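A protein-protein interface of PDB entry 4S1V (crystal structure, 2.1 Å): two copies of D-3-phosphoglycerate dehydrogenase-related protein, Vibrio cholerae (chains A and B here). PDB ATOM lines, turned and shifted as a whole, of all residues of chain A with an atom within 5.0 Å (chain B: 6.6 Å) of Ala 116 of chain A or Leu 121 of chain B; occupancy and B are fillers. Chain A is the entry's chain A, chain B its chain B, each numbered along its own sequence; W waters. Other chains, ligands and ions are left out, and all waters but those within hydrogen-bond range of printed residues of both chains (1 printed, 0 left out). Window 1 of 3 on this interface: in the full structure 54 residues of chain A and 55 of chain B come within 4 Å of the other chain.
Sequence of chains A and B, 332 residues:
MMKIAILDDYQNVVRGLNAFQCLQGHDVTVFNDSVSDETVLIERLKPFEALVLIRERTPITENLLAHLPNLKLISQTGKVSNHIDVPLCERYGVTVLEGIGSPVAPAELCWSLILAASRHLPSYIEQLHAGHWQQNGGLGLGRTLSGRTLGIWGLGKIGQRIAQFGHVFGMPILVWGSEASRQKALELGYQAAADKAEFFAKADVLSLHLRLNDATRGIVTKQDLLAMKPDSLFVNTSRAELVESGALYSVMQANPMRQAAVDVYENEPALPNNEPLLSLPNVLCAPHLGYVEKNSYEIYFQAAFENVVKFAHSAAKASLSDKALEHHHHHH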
ATOM      1  N   LEU A 109      -3.316  13.656 -25.512  1.00  0.00           N
ATOM      2  CA  LEU A 109      -3.002  14.479 -24.348  1.00  0.00           C
ATOM      3  C   LEU A 109      -1.725  15.294 -24.564  1.00  0.00           C
ATOM      4  O   LEU A 109      -1.697  16.490 -24.261  1.00  0.00           O
ATOM      5  CB  LEU A 109      -2.906  13.620 -23.078  1.00  0.00           C
ATOM      6  CG  LEU A 109      -2.756  14.230 -21.673  1.00  0.00           C
ATOM      7  CD1 LEU A 109      -1.326  14.713 -21.397  1.00  0.00           C
ATOM      8  CD2 LEU A 109      -3.783  15.329 -21.400  1.00  0.00           C
ATOM      9  N   SER A 112      -2.577  18.038 -26.779  1.00  0.00           N
ATOM     10  CA  SER A 112      -3.393  19.080 -26.158  1.00  0.00           C
ATOM     11  C   SER A 112      -2.532  20.019 -25.310  1.00  0.00           C
ATOM     12  O   SER A 112      -2.824  21.207 -25.226  1.00  0.00           O
ATOM     13  CB  SER A 112      -4.548  18.492 -25.336  1.00  0.00           C
ATOM     14  OG  SER A 112      -4.086  17.933 -24.119  1.00  0.00           O
ATOM     15  N   LEU A 113      -1.476  19.485 -24.698  1.00  0.00           N
ATOM     16  CA  LEU A 113      -0.565  20.300 -23.886  1.00  0.00           C
ATOM     17  C   LEU A 113       0.291  21.203 -24.754  1.00  0.00           C
ATOM     18  O   LEU A 113       0.629  22.324 -24.346  1.00  0.00           O
ATOM     19  CB  LEU A 113       0.365  19.434 -23.022  1.00  0.00           C
ATOM     20  CG  LEU A 113      -0.148  18.542 -21.903  1.00  0.00           C
ATOM     21  CD1 LEU A 113       1.015  18.044 -21.057  1.00  0.00           C
ATOM     22  CD2 LEU A 113      -1.167  19.248 -21.029  1.00  0.00           C
ATOM     23  N   ILE A 114       0.643  20.702 -25.937  1.00  0.00           N
ATOM     24  CA  ILE A 114       1.433  21.444 -26.916  1.00  0.00           C
ATOM     25  C   ILE A 114       0.662  22.672 -27.393  1.00  0.00           C
ATOM     26  O   ILE A 114       1.226  23.768 -27.462  1.00  0.00           O
ATOM     27  CB  ILE A 114       1.846  20.555 -28.117  1.00  0.00           C
ATOM     28  CG1 ILE A 114       2.968  19.597 -27.696  1.00  0.00           C
ATOM     29  CG2 ILE A 114       2.294  21.407 -29.300  1.00  0.00           C
ATOM     30  CD1 ILE A 114       3.355  18.563 -28.731  1.00  0.00           C
ATOM     31  N   LEU A 115      -0.622  22.479 -27.712  1.00  0.00           N
ATOM     32  CA  LEU A 115      -1.486  23.578 -28.131  1.00  0.00           C
ATOM     33  C   LEU A 115      -1.778  24.525 -26.974  1.00  0.00           C
ATOM     34  O   LEU A 115      -1.726  25.745 -27.146  1.00  0.00           O
ATOM     35  CB  LEU A 115      -2.798  23.059 -28.726  1.00  0.00           C
ATOM     36  CG  LEU A 115      -2.774  22.543 -30.165  1.00  0.00           C
ATOM     37  CD1 LEU A 115      -4.095  21.880 -30.509  1.00  0.00           C
ATOM     38  CD2 LEU A 115      -2.491  23.668 -31.149  1.00  0.00           C
ATOM     39  N   ALA A 116      -2.094  23.963 -25.806  1.00  0.00           N
ATOM     40  CA  ALA A 116      -2.433  24.768 -24.627  1.00  0.00           C
ATOM     41  C   ALA A 116      -1.275  25.664 -24.200  1.00  0.00           C
ATOM     42  O   ALA A 116      -1.475  26.846 -23.880  1.00  0.00           O
ATOM     43  CB  ALA A 116      -2.874  23.879 -23.472  1.00  0.00           C
ATOM     44  N   ALA A 117      -0.069  25.097 -24.207  1.00  0.00           N
ATOM     45  CA  ALA A 117       1.147  25.845 -23.892  1.00  0.00           C
ATOM     46  C   ALA A 117       1.400  26.922 -24.949  1.00  0.00           C
ATOM     47  O   ALA A 117       1.568  28.083 -24.609  1.00  0.00           O
ATOM     48  CB  ALA A 117       2.339  24.906 -23.780  1.00  0.00           C
ATOM     49  N   SER A 118       1.397  26.527 -26.223  1.00  0.00           N
ATOM     50  CA  SER A 118       1.603  27.447 -27.358  1.00  0.00           C
ATOM     51  C   SER A 118       0.658  28.650 -27.352  1.00  0.00           C
ATOM     52  O   SER A 118       1.028  29.722 -27.816  1.00  0.00           O
ATOM     53  CB  SER A 118       1.448  26.715 -28.692  1.00  0.00           C
ATOM     54  OG  SER A 118       2.338  25.617 -28.804  1.00  0.00           O
ATOM     55  N   ARG A 119      -0.554  28.466 -26.838  1.00  0.00           N
ATOM     56  CA  ARG A 119      -1.553  29.543 -26.806  1.00  0.00           C
ATOM     57  C   ARG A 119      -1.871  30.102 -25.405  1.00  0.00           C
ATOM     58  O   ARG A 119      -2.733  30.974 -25.278  1.00  0.00           O
ATOM     59  CB  ARG A 119      -2.848  29.093 -27.503  1.00  0.00           C
ATOM     60  CG  ARG A 119      -2.677  28.697 -28.969  1.00  0.00           C
ATOM     61  CD  ARG A 119      -2.093  29.824 -29.824  1.00  0.00           C
ATOM     62  NE  ARG A 119      -3.071  30.891 -30.027  1.00  0.00           N
ATOM     63  CZ  ARG A 119      -3.883  30.985 -31.076  1.00  0.00           C
ATOM     64  NH1 ARG A 119      -3.834  30.082 -32.054  1.00  0.00           N
ATOM     65  NH2 ARG A 119      -4.739  31.994 -31.151  1.00  0.00           N
ATOM     66  N   HIS A 120      -1.181  29.600 -24.374  1.00  0.00           N
ATOM     67  CA  HIS A 120      -1.386  30.023 -22.982  1.00  0.00           C
ATOM     68  C   HIS A 120      -2.832  29.950 -22.581  1.00  0.00           C
ATOM     69  O   HIS A 120      -3.328  30.823 -21.880  1.00  0.00           O
ATOM     70  CB  HIS A 120      -0.816  31.427 -22.729  1.00  0.00           C
ATOM     71  CG  HIS A 120       0.565  31.628 -23.293  1.00  0.00           C
ATOM     72  ND1 HIS A 120       1.610  30.862 -22.934  1.00  0.00           N
ATOM     73  CD2 HIS A 120       1.041  32.523 -24.245  1.00  0.00           C
ATOM     74  CE1 HIS A 120       2.706  31.249 -23.605  1.00  0.00           C
ATOM     75  NE2 HIS A 120       2.362  32.268 -24.411  1.00  0.00           N
ATOM     76  N   LEU A 121      -3.500  28.888 -23.026  1.00  0.00           N
ATOM     77  CA  LEU A 121      -4.939  28.696 -22.839  1.00  0.00           C
ATOM     78  C   LEU A 121      -5.436  28.610 -21.383  1.00  0.00           C
ATOM     79  O   LEU A 121      -6.374  29.325 -21.028  1.00  0.00           O
ATOM     80  CB  LEU A 121      -5.416  27.484 -23.642  1.00  0.00           C
ATOM     81  CG  LEU A 121      -6.914  27.175 -23.664  1.00  0.00           C
ATOM     82  CD1 LEU A 121      -7.732  28.334 -24.231  1.00  0.00           C
ATOM     83  CD2 LEU A 121      -7.156  25.895 -24.453  1.00  0.00           C
ATOM     84  N   PRO A 122      -4.827  27.739 -20.544  1.00  0.00           N
ATOM     85  CA  PRO A 122      -5.298  27.664 -19.155  1.00  0.00           C
ATOM     86  C   PRO A 122      -5.201  28.999 -18.425  1.00  0.00           C
ATOM     87  O   PRO A 122      -6.085  29.317 -17.637  1.00  0.00           O
ATOM     88  CB  PRO A 122      -4.355  26.637 -18.508  1.00  0.00           C
ATOM     89  CG  PRO A 122      -3.817  25.842 -19.643  1.00  0.00           C
ATOM     90  CD  PRO A 122      -3.702  26.815 -20.781  1.00  0.00           C
ATOM     91  N   LEU A 284       3.927  24.809 -18.185  1.00  0.00           N
ATOM     92  CA  LEU A 284       2.572  24.264 -18.077  1.00  0.00           C
ATOM     93  C   LEU A 284       2.649  22.863 -17.465  1.00  0.00           C
ATOM     94  O   LEU A 284       3.257  21.968 -18.039  1.00  0.00           O
ATOM     95  CB  LEU A 284       1.895  24.231 -19.455  1.00  0.00           C
ATOM     96  CG  LEU A 284       0.516  23.572 -19.608  1.00  0.00           C
ATOM     97  CD1 LEU A 284      -0.259  24.242 -20.724  1.00  0.00           C
ATOM     98  CD2 LEU A 284       0.626  22.077 -19.878  1.00  0.00           C
ATOM     99  N   ALA A 286       0.768  19.427 -15.981  1.00  0.00           N
ATOM    100  CA  ALA A 286      -0.422  18.580 -15.939  1.00  0.00           C
ATOM    101  C   ALA A 286      -0.159  17.380 -15.026  1.00  0.00           C
ATOM    102  O   ALA A 286       0.974  16.904 -14.953  1.00  0.00           O
ATOM    103  CB  ALA A 286      -0.800  18.131 -17.348  1.00  0.00           C
ATOM    104  N   LEU A 289      -1.705  13.017 -16.909  1.00  0.00           N
ATOM    105  CA  LEU A 289      -2.992  12.709 -17.508  1.00  0.00           C
ATOM    106  C   LEU A 289      -2.914  12.035 -18.879  1.00  0.00           C
ATOM    107  O   LEU A 289      -3.886  12.062 -19.620  1.00  0.00           O
ATOM    108  CB  LEU A 289      -3.695  14.014 -17.882  1.00  0.00           C
ATOM    109  CG  LEU A 289      -4.155  14.888 -16.714  1.00  0.00           C
ATOM    110  CD1 LEU A 289      -4.700  16.203 -17.246  1.00  0.00           C
ATOM    111  CD2 LEU A 289      -5.205  14.141 -15.898  1.00  0.00           C
ATOM    112  N   SER B 112      -7.426  23.515 -30.042  1.00  0.00           N
ATOM    113  CA  SER B 112      -6.930  23.577 -28.674  1.00  0.00           C
ATOM    114  C   SER B 112      -8.078  23.570 -27.657  1.00  0.00           C
ATOM    115  O   SER B 112      -7.969  22.954 -26.592  1.00  0.00           O
ATOM    116  CB  SER B 112      -6.066  24.826 -28.488  1.00  0.00           C
ATOM    117  OG  SER B 112      -5.558  24.893 -27.169  1.00  0.00           O
ATOM    118  N   LEU B 115      -9.629  19.952 -27.629  1.00  0.00           N
ATOM    119  CA  LEU B 115      -8.784  19.027 -26.877  1.00  0.00           C
ATOM    120  C   LEU B 115      -8.766  19.320 -25.384  1.00  0.00           C
ATOM    121  O   LEU B 115      -8.817  18.392 -24.582  1.00  0.00           O
ATOM    122  CB  LEU B 115      -7.364  19.010 -27.438  1.00  0.00           C
ATOM    123  CG  LEU B 115      -7.100  18.223 -28.720  1.00  0.00           C
ATOM    124  CD1 LEU B 115      -5.771  18.671 -29.318  1.00  0.00           C
ATOM    125  CD2 LEU B 115      -7.093  16.715 -28.478  1.00  0.00           C
ATOM    126  N   ALA B 116      -8.709  20.604 -25.015  1.00  0.00           N
ATOM    127  CA  ALA B 116      -8.754  21.015 -23.603  1.00  0.00           C
ATOM    128  C   ALA B 116     -10.075  20.622 -22.933  1.00  0.00           C
ATOM    129  O   ALA B 116     -10.090  20.096 -21.817  1.00  0.00           O
ATOM    130  CB  ALA B 116      -8.528  22.515 -23.469  1.00  0.00           C
ATOM    131  N   ALA B 117     -11.175  20.892 -23.625  1.00  0.00           N
ATOM    132  CA  ALA B 117     -12.509  20.554 -23.141  1.00  0.00           C
ATOM    133  C   ALA B 117     -12.657  19.044 -22.981  1.00  0.00           C
ATOM    134  O   ALA B 117     -13.154  18.564 -21.964  1.00  0.00           O
ATOM    135  CB  ALA B 117     -13.565  21.100 -24.093  1.00  0.00           C
ATOM    136  N   SER B 118     -12.202  18.304 -23.986  1.00  0.00           N
ATOM    137  CA  SER B 118     -12.314  16.848 -23.990  1.00  0.00           C
ATOM    138  C   SER B 118     -11.579  16.241 -22.812  1.00  0.00           C
ATOM    139  O   SER B 118     -12.049  15.278 -22.221  1.00  0.00           O
ATOM    140  CB  SER B 118     -11.773  16.257 -25.291  1.00  0.00           C
ATOM    141  OG  SER B 118     -12.603  16.606 -26.379  1.00  0.00           O
ATOM    142  N   ARG B 119     -10.434  16.811 -22.457  1.00  0.00           N
ATOM    143  CA  ARG B 119      -9.615  16.190 -21.428  1.00  0.00           C
ATOM    144  C   ARG B 119      -9.670  16.888 -20.071  1.00  0.00           C
ATOM    145  O   ARG B 119      -8.929  16.511 -19.163  1.00  0.00           O
ATOM    146  CB  ARG B 119      -8.175  15.995 -21.923  1.00  0.00           C
ATOM    147  CG  ARG B 119      -8.052  15.111 -23.164  1.00  0.00           C
ATOM    148  CD  ARG B 119      -8.411  13.643 -22.912  1.00  0.00           C
ATOM    149  NE  ARG B 119      -7.410  12.967 -22.089  1.00  0.00           N
ATOM    150  CZ  ARG B 119      -6.399  12.237 -22.555  1.00  0.00           C
ATOM    151  NH1 ARG B 119      -6.235  12.044 -23.861  1.00  0.00           N
ATOM    152  NH2 ARG B 119      -5.556  11.677 -21.700  1.00  0.00           N
ATOM    153  N   HIS B 120     -10.578  17.863 -19.937  1.00  0.00           N
ATOM    154  CA  HIS B 120     -10.744  18.671 -18.715  1.00  0.00           C
ATOM    155  C   HIS B 120      -9.469  19.309 -18.267  1.00  0.00           C
ATOM    156  O   HIS B 120      -9.197  19.420 -17.070  1.00  0.00           O
ATOM    157  CB  HIS B 120     -11.354  17.852 -17.581  1.00  0.00           C
ATOM    158  CG  HIS B 120     -12.676  17.227 -17.933  1.00  0.00           C
ATOM    159  ND1 HIS B 120     -13.737  17.956 -18.315  1.00  0.00           N
ATOM    160  CD2 HIS B 120     -13.084  15.893 -17.944  1.00  0.00           C
ATOM    161  CE1 HIS B 120     -14.779  17.133 -18.558  1.00  0.00           C
ATOM    162  NE2 HIS B 120     -14.372  15.870 -18.333  1.00  0.00           N
ATOM    163  N   LEU B 121      -8.677  19.747 -19.239  1.00  0.00           N
ATOM    164  CA  LEU B 121      -7.328  20.203 -18.970  1.00  0.00           C
ATOM    165  C   LEU B 121      -7.223  21.409 -18.002  1.00  0.00           C
ATOM    166  O   LEU B 121      -6.412  21.365 -17.069  1.00  0.00           O
ATOM    167  CB  LEU B 121      -6.596  20.455 -20.290  1.00  0.00           C
ATOM    168  CG  LEU B 121      -5.083  20.604 -20.212  1.00  0.00           C
ATOM    169  CD1 LEU B 121      -4.438  19.330 -19.675  1.00  0.00           C
ATOM    170  CD2 LEU B 121      -4.543  20.996 -21.581  1.00  0.00           C
ATOM    171  N   PRO B 122      -8.043  22.471 -18.198  1.00  0.00           N
ATOM    172  CA  PRO B 122      -7.881  23.629 -17.304  1.00  0.00           C
ATOM    173  C   PRO B 122      -8.179  23.327 -15.827  1.00  0.00           C
ATOM    174  O   PRO B 122      -7.443  23.787 -14.952  1.00  0.00           O
ATOM    175  CB  PRO B 122      -8.882  24.660 -17.859  1.00  0.00           C
ATOM    176  CG  PRO B 122      -9.186  24.211 -19.252  1.00  0.00           C
ATOM    177  CD  PRO B 122      -9.093  22.714 -19.209  1.00  0.00           C
ATOM    178  N   SER B 123      -9.233  22.550 -15.565  1.00  0.00           N
ATOM    179  CA  SER B 123      -9.606  22.175 -14.195  1.00  0.00           C
ATOM    180  C   SER B 123      -8.563  21.268 -13.546  1.00  0.00           C
ATOM    181  O   SER B 123      -8.260  21.422 -12.370  1.00  0.00           O
ATOM    182  CB  SER B 123     -10.971  21.478 -14.161  1.00  0.00           C
ATOM    183  OG  SER B 123     -11.946  22.247 -14.832  1.00  0.00           O
ATOM    184  N   TYR B 124      -8.049  20.305 -14.309  1.00  0.00           N
ATOM    185  CA  TYR B 124      -6.987  19.420 -13.826  1.00  0.00           C
ATOM    186  C   TYR B 124      -5.765  20.239 -13.402  1.00  0.00           C
ATOM    187  O   TYR B 124      -5.238  20.060 -12.306  1.00  0.00           O
ATOM    188  CB  TYR B 124      -6.583  18.400 -14.903  1.00  0.00           C
ATOM    189  CG  TYR B 124      -7.317  17.063 -14.883  1.00  0.00           C
ATOM    190  CD1 TYR B 124      -7.340  16.267 -13.735  1.00  0.00           C
ATOM    191  CD2 TYR B 124      -7.940  16.575 -16.029  1.00  0.00           C
ATOM    192  CE1 TYR B 124      -7.976  15.035 -13.724  1.00  0.00           C
ATOM    193  CE2 TYR B 124      -8.584  15.340 -16.032  1.00  0.00           C
ATOM    194  CZ  TYR B 124      -8.601  14.574 -14.878  1.00  0.00           C
ATOM    195  OH  TYR B 124      -9.233  13.356 -14.879  1.00  0.00           O
ATOM    196  N   ILE B 125      -5.334  21.134 -14.291  1.00  0.00           N
ATOM    197  CA  ILE B 125      -4.200  22.025 -14.064  1.00  0.00           C
ATOM    198  C   ILE B 125      -4.429  22.941 -12.856  1.00  0.00           C
ATOM    199  O   ILE B 125      -3.583  23.022 -11.965  1.00  0.00           O
ATOM    200  CB  ILE B 125      -3.879  22.832 -15.347  1.00  0.00           C
ATOM    201  CG1 ILE B 125      -3.291  21.888 -16.405  1.00  0.00           C
ATOM    202  CG2 ILE B 125      -2.929  23.994 -15.055  1.00  0.00           C
ATOM    203  CD1 ILE B 125      -3.289  22.443 -17.811  1.00  0.00           C
ATOM    204  N   GLU B 126      -5.583  23.599 -12.812  1.00  0.00           N
ATOM    205  CA  GLU B 126      -5.919  24.477 -11.685  1.00  0.00           C
ATOM    206  C   GLU B 126      -5.939  23.746 -10.336  1.00  0.00           C
ATOM    207  O   GLU B 126      -5.463  24.282  -9.329  1.00  0.00           O
ATOM    208  CB  GLU B 126      -7.255  25.172 -11.938  1.00  0.00           C
ATOM    209  CG  GLU B 126      -7.695  26.128 -10.846  1.00  0.00           C
ATOM    210  CD  GLU B 126      -9.169  26.458 -10.960  1.00  0.00           C
ATOM    211  OE1 GLU B 126      -9.535  27.244 -11.861  1.00  0.00           O
ATOM    212  OE2 GLU B 126      -9.964  25.919 -10.159  1.00  0.00           O
ATOM    213  N   LEU B 284     -16.234  25.317 -21.308  1.00  0.00           N
ATOM    214  CA  LEU B 284     -14.933  25.944 -21.404  1.00  0.00           C
ATOM    215  C   LEU B 284     -15.123  27.301 -22.074  1.00  0.00           C
ATOM    216  O   LEU B 284     -15.681  27.387 -23.169  1.00  0.00           O
ATOM    217  CB  LEU B 284     -13.954  25.046 -22.182  1.00  0.00           C
ATOM    218  CG  LEU B 284     -12.479  25.469 -22.262  1.00  0.00           C
ATOM    219  CD1 LEU B 284     -11.566  24.266 -22.410  1.00  0.00           C
ATOM    220  CD2 LEU B 284     -12.218  26.471 -23.388  1.00  0.00           C
HETATM  221  O   HOH W   1      -5.422  22.204 -25.641  1.00  0.00           O
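Water W1 lies within hydrogen-bond range of the backbone carbonyl oxygen of Ser 112 of chain A (2.8 Å) and the backbone carbonyl oxygen of Ser 112 of chain B (2.8 Å).
O of Leu 289 of chain A is in hydrogen-bond range of NH2 of Arg 119 of chain B (2.7 Å).
CB of Leu 109 of chain A touches NH2 of Arg 119 of chain B, 3.6 Å away.
CD2 of Leu 113 of chain A touches CD1 of Leu 121 of chain B, at 3.5 Å.
Leu 115 of chain A touches Ser 112 of chain B (CB to OG, 3.7 Å).
CD1 of Leu 115 of chain A touches CD1 of Leu 115 of chain B, 3.8 Å away.
Ala 116 of chain A touches Ser 112 of chain B.
Leu 121 of chain B touches Ala 116 of chain A.
Ser 112 of chain B touches Leu 121 of chain A.
Ile 125 of chain B touches Pro 122 of chain A (CD1 to CG, 3.9 Å).
CD1 of Leu 289 of chain A touches CD1 of Leu 121 of chain B, 3.97 Å away.
CD2 of Tyr 124 of chain B touches CD1 of Leu 289 of chain A, at 3.5 Å.
Printed residues of chain A that touch a printed residue of chain B: Leu 109, Ser 112, Leu 113, Leu 115, Ala 116, Leu 121, Pro 122 and Leu 289.
Of the 14 printed residues of chain B, 7 touch a printed residue of chain A.
Printed residues of chain B that touch a printed residue of chain A: Ser 112, Leu 115, Ala 116, Arg 119, Leu 121, Tyr 124 and Ile 125.
Hydrophobic or aromatic side chains of chain B that line the printed part of chain A: Leu 115, Ala 116, Leu 121, Tyr 124 and Ile 125.
Among the printed residues, 13 pairs touch across the chains.
Among the printed residues, no Asp or Glu carboxylate lies within 4 Å of a Lys or Arg side-chain nitrogen of the other chain.
Leu 115 of chain B touches its own counterpart, Leu 115 of chain A.
Ala 116 of chain A touches Ser 112 of chain B, but with the chains exchanged Ser 112 of chain A does not touch Ala 116 of chain B (4.7 Å).
Ala 116 of chain A touches Leu 121 of chain B, and with the chains exchanged Leu 121 of chain A touches Ala 116 of chain B.
Leu 121 of chain A touches Ser 112 of chain B, but with the chains exchanged Ser 112 of chain A does not touch Leu 121 of chain B (4.004 Å).
Of the 13 pairs that touch across the chains among the printed residues, 5 have their exchanged pair printed and touching as well.
N of Leu 121 of chain A sits at hydrogen-bond distance from O of Ala 116 of chain A, at 3.0 Å.
The side-chain hydroxyl (OG) of Ser 112 of chain A is in hydrogen-bond range of the backbone carbonyl oxygen (O) of Leu 109 of chain A, at 2.8 Å.
The backbone carbonyl oxygen of Ala 116 of chain B sits at hydrogen-bond distance from the backbone NH of Leu 121 of chain B (3.0 Å).
Ala 116 of chain A touches two residues of chain B.
Of the printed residues of chain A, Leu 121 of chain B touches Leu 113, Ala 116 and Leu 289.
Of the printed residues of chain B, Leu 109 of chain A touches Arg 119.
Of the printed residues of chain A, Tyr 124 of chain B touches Leu 289 (3.5 Å).
Pro 122 of chain B touches none of the printed residues of chain A.
Leu 284 of chain A touches none of the printed residues of chain B.
The nearest residue of chain B that does not touch Ala 116 of chain A is Ala 116 of chain B (5.8 Å).
The nearest printed residue of chain A that does not touch Leu 121 of chain B is Ser 112 of chain A (4.004 Å).
The nearest printed residue of chain B that does not touch Leu 121 of chain A is Leu 284 of chain B (4.9 Å).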
